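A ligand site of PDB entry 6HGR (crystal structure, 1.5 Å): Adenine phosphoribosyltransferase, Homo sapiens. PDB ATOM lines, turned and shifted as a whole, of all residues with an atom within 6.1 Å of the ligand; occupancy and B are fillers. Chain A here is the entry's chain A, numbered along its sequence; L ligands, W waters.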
ATOM      1  N   PHE A  17      -7.241  37.211   0.531  1.00  0.00           N
ATOM      2  CA  PHE A  17      -6.019  36.605  -0.015  1.00  0.00           C
ATOM      3  C   PHE A  17      -6.358  35.851  -1.293  1.00  0.00           C
ATOM      4  O   PHE A  17      -7.261  35.016  -1.278  1.00  0.00           O
ATOM      5  CB  PHE A  17      -5.401  35.607   0.978  1.00  0.00           C
ATOM      6  CG  PHE A  17      -4.089  35.053   0.512  1.00  0.00           C
ATOM      7  CD1 PHE A  17      -2.919  35.759   0.717  1.00  0.00           C
ATOM      8  CD2 PHE A  17      -4.030  33.851  -0.182  1.00  0.00           C
ATOM      9  CE1 PHE A  17      -1.705  35.279   0.265  1.00  0.00           C
ATOM     10  CE2 PHE A  17      -2.820  33.367  -0.651  1.00  0.00           C
ATOM     11  CZ  PHE A  17      -1.652  34.081  -0.423  1.00  0.00           C
ATOM     12  N   VAL A  23     -11.903  34.927  -0.759  1.00  0.00           N
ATOM     13  CA  VAL A  23     -11.626  34.095   0.386  1.00  0.00           C
ATOM     14  C   VAL A  23     -10.823  32.899  -0.091  1.00  0.00           C
ATOM     15  O   VAL A  23     -11.291  32.135  -0.929  1.00  0.00           O
ATOM     16  CB  VAL A  23     -12.929  33.658   1.086  1.00  0.00           C
ATOM     17  CG1 VAL A  23     -12.630  32.731   2.248  1.00  0.00           C
ATOM     18  CG2 VAL A  23     -13.692  34.888   1.563  1.00  0.00           C
ATOM     19  N   PHE A  24      -9.629  32.723   0.459  1.00  0.00           N
ATOM     20  CA  PHE A  24      -8.746  31.645   0.043  1.00  0.00           C
ATOM     21  C   PHE A  24      -9.048  30.422   0.881  1.00  0.00           C
ATOM     22  O   PHE A  24      -9.040  30.493   2.099  1.00  0.00           O
ATOM     23  CB  PHE A  24      -7.288  32.077   0.235  1.00  0.00           C
ATOM     24  CG  PHE A  24      -6.289  31.071  -0.253  1.00  0.00           C
ATOM     25  CD1 PHE A  24      -5.867  30.039   0.566  1.00  0.00           C
ATOM     26  CD2 PHE A  24      -5.758  31.179  -1.520  1.00  0.00           C
ATOM     27  CE1 PHE A  24      -4.937  29.113   0.112  1.00  0.00           C
ATOM     28  CE2 PHE A  24      -4.818  30.273  -1.975  1.00  0.00           C
ATOM     29  CZ  PHE A  24      -4.409  29.239  -1.152  1.00  0.00           C
ATOM     30  N   ARG A  25      -9.317  29.283   0.250  1.00  0.00           N
ATOM     31  CA  ARG A  25      -9.540  28.053   1.001  1.00  0.00           C
ATOM     32  C   ARG A  25      -8.244  27.262   1.101  1.00  0.00           C
ATOM     33  O   ARG A  25      -7.709  26.816   0.092  1.00  0.00           O
ATOM     34  CB  ARG A  25     -10.607  27.193   0.329  1.00  0.00           C
ATOM     35  CG  ARG A  25     -11.854  27.965  -0.042  1.00  0.00           C
ATOM     36  CD  ARG A  25     -12.597  28.486   1.162  1.00  0.00           C
ATOM     37  NE  ARG A  25     -13.691  29.362   0.732  1.00  0.00           N
ATOM     38  CZ  ARG A  25     -14.652  29.807   1.514  1.00  0.00           C
ATOM     39  NH1 ARG A  25     -14.705  29.496   2.793  1.00  0.00           N
ATOM     40  NH2 ARG A  25     -15.596  30.596   0.993  1.00  0.00           N
ATOM     41  N   ASP A  26      -7.742  27.115   2.325  1.00  0.00           N
ATOM     42  CA  ASP A  26      -6.440  26.492   2.565  1.00  0.00           C
ATOM     43  C   ASP A  26      -6.664  25.038   2.962  1.00  0.00           C
ATOM     44  O   ASP A  26      -7.264  24.760   4.000  1.00  0.00           O
ATOM     45  CB  ASP A  26      -5.737  27.260   3.691  1.00  0.00           C
ATOM     46  CG  ASP A  26      -4.373  26.684   4.063  1.00  0.00           C
ATOM     47  OD1 ASP A  26      -3.782  25.934   3.249  1.00  0.00           O
ATOM     48  OD2 ASP A  26      -3.885  27.029   5.164  1.00  0.00           O
ATOM     49  N   ILE A  27      -6.202  24.128   2.128  1.00  0.00           N
ATOM     50  CA  ILE A  27      -6.319  22.689   2.390  1.00  0.00           C
ATOM     51  C   ILE A  27      -5.150  22.121   3.190  1.00  0.00           C
ATOM     52  O   ILE A  27      -5.150  20.936   3.536  1.00  0.00           O
ATOM     53  CB  ILE A  27      -6.531  21.904   1.068  1.00  0.00           C
ATOM     54  CG1 ILE A  27      -5.420  22.205   0.052  1.00  0.00           C
ATOM     55  CG2 ILE A  27      -7.884  22.279   0.473  1.00  0.00           C
ATOM     56  CD1 ILE A  27      -4.149  21.393   0.230  1.00  0.00           C
ATOM     57  N   LEU A  62      -2.433  17.249 -11.138  1.00  0.00           N
ATOM     58  CA  LEU A  62      -2.005  18.581 -11.570  1.00  0.00           C
ATOM     59  C   LEU A  62      -0.983  19.238 -10.634  1.00  0.00           C
ATOM     60  O   LEU A  62      -1.169  19.308  -9.415  1.00  0.00           O
ATOM     61  CB  LEU A  62      -3.195  19.520 -11.708  1.00  0.00           C
ATOM     62  CG  LEU A  62      -4.273  19.037 -12.684  1.00  0.00           C
ATOM     63  CD1 LEU A  62      -5.251  20.157 -13.038  1.00  0.00           C
ATOM     64  CD2 LEU A  62      -3.644  18.444 -13.933  1.00  0.00           C
ATOM     65  N   ASP A  63       0.112  19.703 -11.214  1.00  0.00           N
ATOM     66  CA  ASP A  63       1.094  20.538 -10.514  1.00  0.00           C
ATOM     67  C   ASP A  63       0.412  21.784  -9.958  1.00  0.00           C
ATOM     68  O   ASP A  63      -0.328  22.437 -10.700  1.00  0.00           O
ATOM     69  CB  ASP A  63       2.134  20.973 -11.545  1.00  0.00           C
ATOM     70  CG  ASP A  63       3.455  21.387 -10.945  1.00  0.00           C
ATOM     71  OD1 ASP A  63       3.549  21.523  -9.704  1.00  0.00           O
ATOM     72  OD2 ASP A  63       4.403  21.578 -11.745  1.00  0.00           O
ATOM     73  N   SER A  64       0.616  22.139  -8.676  1.00  0.00           N
ATOM     74  CA  SER A  64       1.415  21.363  -7.729  1.00  0.00           C
ATOM     75  C   SER A  64       0.571  20.724  -6.632  1.00  0.00           C
ATOM     76  O   SER A  64       0.972  19.736  -6.008  1.00  0.00           O
ATOM     77  CB  SER A  64       2.446  22.286  -7.069  1.00  0.00           C
ATOM     78  OG  SER A  64       3.427  21.532  -6.402  1.00  0.00           O
ATOM     79  N   ARG A  65      -0.592  21.302  -6.327  1.00  0.00           N
ATOM     80  CA  ARG A  65      -1.361  20.767  -5.194  1.00  0.00           C
ATOM     81  C   ARG A  65      -2.132  19.495  -5.578  1.00  0.00           C
ATOM     82  O   ARG A  65      -2.473  18.709  -4.702  1.00  0.00           O
ATOM     83  CB  ARG A  65      -2.254  21.822  -4.549  1.00  0.00           C
ATOM     84  CG  ARG A  65      -1.495  22.831  -3.699  1.00  0.00           C
ATOM     85  CD  ARG A  65      -2.427  23.742  -2.911  1.00  0.00           C
ATOM     86  NE  ARG A  65      -2.976  24.823  -3.728  1.00  0.00           N
ATOM     87  CZ  ARG A  65      -2.660  26.115  -3.581  1.00  0.00           C
ATOM     88  NH1 ARG A  65      -1.817  26.495  -2.623  1.00  0.00           N
ATOM     89  NH2 ARG A  65      -3.204  27.023  -4.375  1.00  0.00           N
ATOM     90  N   TYR A  99      -3.030  29.077 -20.809  1.00  0.00           N
ATOM     91  CA  TYR A  99      -4.379  29.401 -20.370  1.00  0.00           C
ATOM     92  C   TYR A  99      -4.355  30.670 -19.535  1.00  0.00           C
ATOM     93  O   TYR A  99      -3.290  31.256 -19.322  1.00  0.00           O
ATOM     94  CB  TYR A  99      -4.976  28.241 -19.557  1.00  0.00           C
ATOM     95  CG  TYR A  99      -4.183  27.897 -18.316  1.00  0.00           C
ATOM     96  CD1 TYR A  99      -2.988  27.192 -18.408  1.00  0.00           C
ATOM     97  CD2 TYR A  99      -4.623  28.271 -17.057  1.00  0.00           C
ATOM     98  CE1 TYR A  99      -2.255  26.870 -17.280  1.00  0.00           C
ATOM     99  CE2 TYR A  99      -3.896  27.953 -15.922  1.00  0.00           C
ATOM    100  CZ  TYR A  99      -2.718  27.261 -16.037  1.00  0.00           C
ATOM    101  OH  TYR A  99      -1.988  26.946 -14.916  1.00  0.00           O
ATOM    102  N   ASP A 125      -7.144  17.766  -8.862  1.00  0.00           N
ATOM    103  CA  ASP A 125      -6.450  18.937  -8.293  1.00  0.00           C
ATOM    104  C   ASP A 125      -7.076  19.189  -6.919  1.00  0.00           C
ATOM    105  O   ASP A 125      -8.123  18.639  -6.600  1.00  0.00           O
ATOM    106  CB  ASP A 125      -6.616  20.153  -9.199  1.00  0.00           C
ATOM    107  CG  ASP A 125      -5.488  21.197  -9.047  1.00  0.00           C
ATOM    108  OD1 ASP A 125      -4.566  21.042  -8.223  1.00  0.00           O
ATOM    109  OD2 ASP A 125      -5.522  22.203  -9.806  1.00  0.00           O
ATOM    110  N   ASP A 126      -6.494  20.088  -6.150  1.00  0.00           N
ATOM    111  CA  ASP A 126      -7.046  20.375  -4.834  1.00  0.00           C
ATOM    112  C   ASP A 126      -8.357  21.163  -4.886  1.00  0.00           C
ATOM    113  O   ASP A 126      -9.256  20.902  -4.087  1.00  0.00           O
ATOM    114  CB  ASP A 126      -5.996  21.066  -3.938  1.00  0.00           C
ATOM    115  CG  ASP A 126      -5.660  22.467  -4.363  1.00  0.00           C
ATOM    116  OD1 ASP A 126      -5.615  22.773  -5.571  1.00  0.00           O
ATOM    117  OD2 ASP A 126      -5.341  23.281  -3.468  1.00  0.00           O
ATOM    118  N   LEU A 127      -8.481  22.087  -5.841  1.00  0.00           N
ATOM    119  CA  LEU A 127      -9.554  23.047  -5.825  1.00  0.00           C
ATOM    120  C   LEU A 127      -9.844  23.525  -7.209  1.00  0.00           C
ATOM    121  O   LEU A 127      -8.917  23.754  -8.007  1.00  0.00           O
ATOM    122  CB  LEU A 127      -9.182  24.216  -4.908  1.00  0.00           C
ATOM    123  CG  LEU A 127     -10.208  25.343  -4.743  1.00  0.00           C
ATOM    124  CD1 LEU A 127     -10.052  25.958  -3.353  1.00  0.00           C
ATOM    125  CD2 LEU A 127     -10.011  26.384  -5.834  1.00  0.00           C
ATOM    126  N   LEU A 128     -11.138  23.591  -7.529  1.00  0.00           N
ATOM    127  CA  LEU A 128     -11.636  24.143  -8.793  1.00  0.00           C
ATOM    128  C   LEU A 128     -12.185  25.529  -8.514  1.00  0.00           C
ATOM    129  O   LEU A 128     -13.112  25.694  -7.721  1.00  0.00           O
ATOM    130  CB  LEU A 128     -12.773  23.281  -9.348  1.00  0.00           C
ATOM    131  CG  LEU A 128     -13.325  23.728 -10.701  1.00  0.00           C
ATOM    132  CD1 LEU A 128     -12.379  23.274 -11.789  1.00  0.00           C
ATOM    133  CD2 LEU A 128     -14.705  23.129 -10.927  1.00  0.00           C
ATOM    134  N   ALA A 129     -11.632  26.532  -9.209  1.00  0.00           N
ATOM    135  CA  ALA A 129     -12.098  27.911  -9.103  1.00  0.00           C
ATOM    136  C   ALA A 129     -12.718  28.290 -10.446  1.00  0.00           C
ATOM    137  O   ALA A 129     -13.823  27.835 -10.748  1.00  0.00           O
ATOM    138  CB  ALA A 129     -10.951  28.817  -8.714  1.00  0.00           C
ATOM    139  N   THR A 130     -11.986  29.015 -11.297  1.00  0.00           N
ATOM    140  CA  THR A 130     -12.531  29.347 -12.617  1.00  0.00           C
ATOM    141  C   THR A 130     -12.608  28.153 -13.560  1.00  0.00           C
ATOM    142  O   THR A 130     -13.359  28.153 -14.549  1.00  0.00           O
ATOM    143  CB  THR A 130     -11.708  30.444 -13.331  1.00  0.00           C
ATOM    144  OG1 THR A 130     -10.440  29.900 -13.739  1.00  0.00           O
ATOM    145  CG2 THR A 130     -11.487  31.669 -12.439  1.00  0.00           C
ATOM    146  N   GLY A 131     -11.817  27.113 -13.263  1.00  0.00           N
ATOM    147  CA  GLY A 131     -11.734  25.956 -14.128  1.00  0.00           C
ATOM    148  C   GLY A 131     -10.708  26.096 -15.242  1.00  0.00           C
ATOM    149  O   GLY A 131     -10.510  25.165 -16.020  1.00  0.00           O
ATOM    150  N   GLY A 132     -10.007  27.213 -15.305  1.00  0.00           N
ATOM    151  CA  GLY A 132      -8.995  27.400 -16.341  1.00  0.00           C
ATOM    152  C   GLY A 132      -7.934  26.307 -16.346  1.00  0.00           C
ATOM    153  O   GLY A 132      -7.550  25.785 -17.401  1.00  0.00           O
ATOM    154  N   THR A 133      -7.422  25.990 -15.156  1.00  0.00           N
ATOM    155  CA  THR A 133      -6.322  25.057 -15.014  1.00  0.00           C
ATOM    156  C   THR A 133      -6.779  23.654 -15.446  1.00  0.00           C
ATOM    157  O   THR A 133      -6.133  22.990 -16.277  1.00  0.00           O
ATOM    158  CB  THR A 133      -5.806  25.050 -13.564  1.00  0.00           C
ATOM    159  OG1 THR A 133      -5.438  26.392 -13.192  1.00  0.00           O
ATOM    160  CG2 THR A 133      -4.583  24.158 -13.440  1.00  0.00           C
ATOM    161  N   MET A 134      -7.907  23.216 -14.913  1.00  0.00           N
ATOM    162  CA  MET A 134      -8.412  21.896 -15.231  1.00  0.00           C
ATOM    163  C   MET A 134      -8.794  21.776 -16.703  1.00  0.00           C
ATOM    164  O   MET A 134      -8.631  20.733 -17.310  1.00  0.00           O
ATOM    165  CB  MET A 134      -9.639  21.604 -14.371  1.00  0.00           C
ATOM    166  CG  MET A 134     -10.043  20.162 -14.372  1.00  0.00           C
ATOM    167  SD  MET A 134      -9.005  19.224 -13.239  1.00  0.00           S
ATOM    168  CE  MET A 134      -9.734  19.643 -11.646  1.00  0.00           C
ATOM    169  N   LEU A 157     -15.437  26.180  -5.905  1.00  0.00           N
ATOM    170  CA  LEU A 157     -15.955  27.527  -5.618  1.00  0.00           C
ATOM    171  C   LEU A 157     -17.083  27.789  -6.624  1.00  0.00           C
ATOM    172  O   LEU A 157     -16.847  28.121  -7.777  1.00  0.00           O
ATOM    173  CB  LEU A 157     -14.828  28.564  -5.747  1.00  0.00           C
ATOM    174  CG  LEU A 157     -13.594  28.260  -4.887  1.00  0.00           C
ATOM    175  CD1 LEU A 157     -12.527  29.340  -4.992  1.00  0.00           C
ATOM    176  CD2 LEU A 157     -13.967  28.021  -3.439  1.00  0.00           C
ATOM    177  N   LEU A 160     -17.973  30.666  -9.240  1.00  0.00           N
ATOM    178  CA  LEU A 160     -17.091  30.905 -10.384  1.00  0.00           C
ATOM    179  C   LEU A 160     -17.403  30.007 -11.578  1.00  0.00           C
ATOM    180  O   LEU A 160     -16.825  30.170 -12.656  1.00  0.00           O
ATOM    181  CB  LEU A 160     -15.618  30.772  -9.977  1.00  0.00           C
ATOM    182  CG  LEU A 160     -15.109  31.615  -8.808  1.00  0.00           C
ATOM    183  CD1 LEU A 160     -13.631  31.391  -8.533  1.00  0.00           C
ATOM    184  CD2 LEU A 160     -15.384  33.109  -9.000  1.00  0.00           C
HETATM  185  P1  LIG L   1      -8.583  27.904 -11.601  1.00  0.00           P
HETATM  186  O1  LIG L   1      -9.131  29.314 -11.530  1.00  0.00           O
HETATM  187  O2  LIG L   1      -9.698  26.879 -11.423  1.00  0.00           O
HETATM  188  O3  LIG L   1      -7.705  27.688 -12.810  1.00  0.00           O
HETATM  189  O4  LIG L   1      -7.636  27.847 -10.335  1.00  0.00           O
HETATM  190  C1  LIG L   1      -7.474  26.604  -9.655  1.00  0.00           C
HETATM  191  C2  LIG L   1      -6.112  26.508  -9.076  1.00  0.00           C
HETATM  192  O5  LIG L   1      -5.534  27.636  -8.466  1.00  0.00           O
HETATM  193  C3  LIG L   1      -5.995  25.199  -8.380  1.00  0.00           C
HETATM  194  O6  LIG L   1      -4.913  24.461  -8.943  1.00  0.00           O
HETATM  195  C4  LIG L   1      -5.636  25.700  -7.002  1.00  0.00           C
HETATM  196  O7  LIG L   1      -4.482  24.969  -6.593  1.00  0.00           O
HETATM  197  C5  LIG L   1      -5.387  27.220  -7.102  1.00  0.00           C
HETATM  198  N1  LIG L   1      -6.384  27.952  -6.308  1.00  0.00           N
HETATM  199  C6  LIG L   1      -7.274  28.856  -6.760  1.00  0.00           C
HETATM  200  N2  LIG L   1      -8.037  29.338  -5.745  1.00  0.00           N
HETATM  201  C7  LIG L   1      -7.606  28.742  -4.606  1.00  0.00           C
HETATM  202  C8  LIG L   1      -7.958  28.792  -3.228  1.00  0.00           C
HETATM  203  O8  LIG L   1      -8.923  29.490  -2.771  1.00  0.00           O
HETATM  204  N3  LIG L   1      -7.294  27.982  -2.355  1.00  0.00           N
HETATM  205  C9  LIG L   1      -6.287  27.200  -2.766  1.00  0.00           C
HETATM  206  N4  LIG L   1      -5.907  27.110  -4.049  1.00  0.00           N
HETATM  207  C10 LIG L   1      -6.554  27.860  -4.973  1.00  0.00           C
HETATM  208  O   HOH W   1      -1.436  25.197  -6.171  1.00  0.00           O
HETATM  209  O   HOH W   2      -8.381  31.418  -9.979  1.00  0.00           O
HETATM  210  O   HOH W   3      -9.104  24.435 -12.588  1.00  0.00           O
HETATM  211  O   HOH W   4     -10.206  31.526  -3.541  1.00  0.00           O
HETATM  212  O   HOH W   5      -7.077  29.676 -14.435  1.00  0.00           O
HETATM  213  O   HOH W   6      -9.507  31.591  -6.746  1.00  0.00           O
HETATM  214  O   HOH W   7      -5.320  25.116  -0.480  1.00  0.00           O
HETATM  215  O   HOH W   8      -2.323  22.267  -8.263  1.00  0.00           O
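Water W4 bridges an oxygen (O8) of the ligand (2.5 Å) and the backbone carbonyl oxygen (O) of Val 23 (2.9 Å). Water W5 lies within hydrogen-bond range of an oxygen (O3) of the ligand (2.6 Å) and the side-chain hydroxyl (OG1) of Thr 130 (3.4 Å). Water W3 lies within hydrogen-bond range of an oxygen (O2) of the ligand, the backbone NH (N) of Met 134 and the backbone NH (N) of Thr 133. Water W1 lies within hydrogen-bond range of the guanidinium group (NE) of Arg 65 (2.9 Å) and an oxygen (O7) of the ligand (3.1 Å).
Val 23 touches the ligand. Phe 24 touches the ligand (CZ to C9, 3.2 Å). Leu 127 touches the ligand (O to C3, 3.3 Å). Of the 23 residues printed, 12 come within 4 Å of the ligand. The nearest printed residue that does not touch the ligand is Leu 128 (4.1 Å).
The backbone NH (N) of Gly 132 is in hydrogen-bond range of an oxygen (O3) of the ligand, 3.4 Å away. O3 of the ligand is in hydrogen-bond range of N of Thr 133 (2.9 Å). The backbone carbonyl oxygen (O) of Arg 25 lies within hydrogen-bond range of a nitrogen (N3) of the ligand, at 2.7 Å. The side-chain carboxylate (OD1) of Asp 126 sits at hydrogen-bond distance from an oxygen (O7) of the ligand. The backbone NH of Thr 130 sits at hydrogen-bond distance from an oxygen (O1) of the ligand. O2 of the ligand is in hydrogen-bond range of N of Ala 129, at 3.0 Å. The side-chain hydroxyl (OG1) of Thr 133 sits at hydrogen-bond distance from an oxygen (O3) of the ligand (2.6 Å). NH2 of Arg 65 is in hydrogen-bond range of N4 of the ligand. An oxygen (O1) of the ligand is in hydrogen-bond range of the side-chain hydroxyl of Thr 130 (2.6 Å). N of Arg 25 is in hydrogen-bond range of O8 of the ligand (3.1 Å). The backbone NH (N) of Gly 131 lies within hydrogen-bond range of an oxygen (O2) of the ligand (2.8 Å). OD2 of Asp 125 is in hydrogen-bond range of O6 of the ligand, 2.5 Å away.
OD2 of Asp 126 lies within salt-bridge range of NE of Arg 65, at 2.8 Å. The side-chain hydroxyl (OG1) of Thr 130 is in hydrogen-bond range of the backbone NH (N) of Gly 132, at 3.1 Å.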
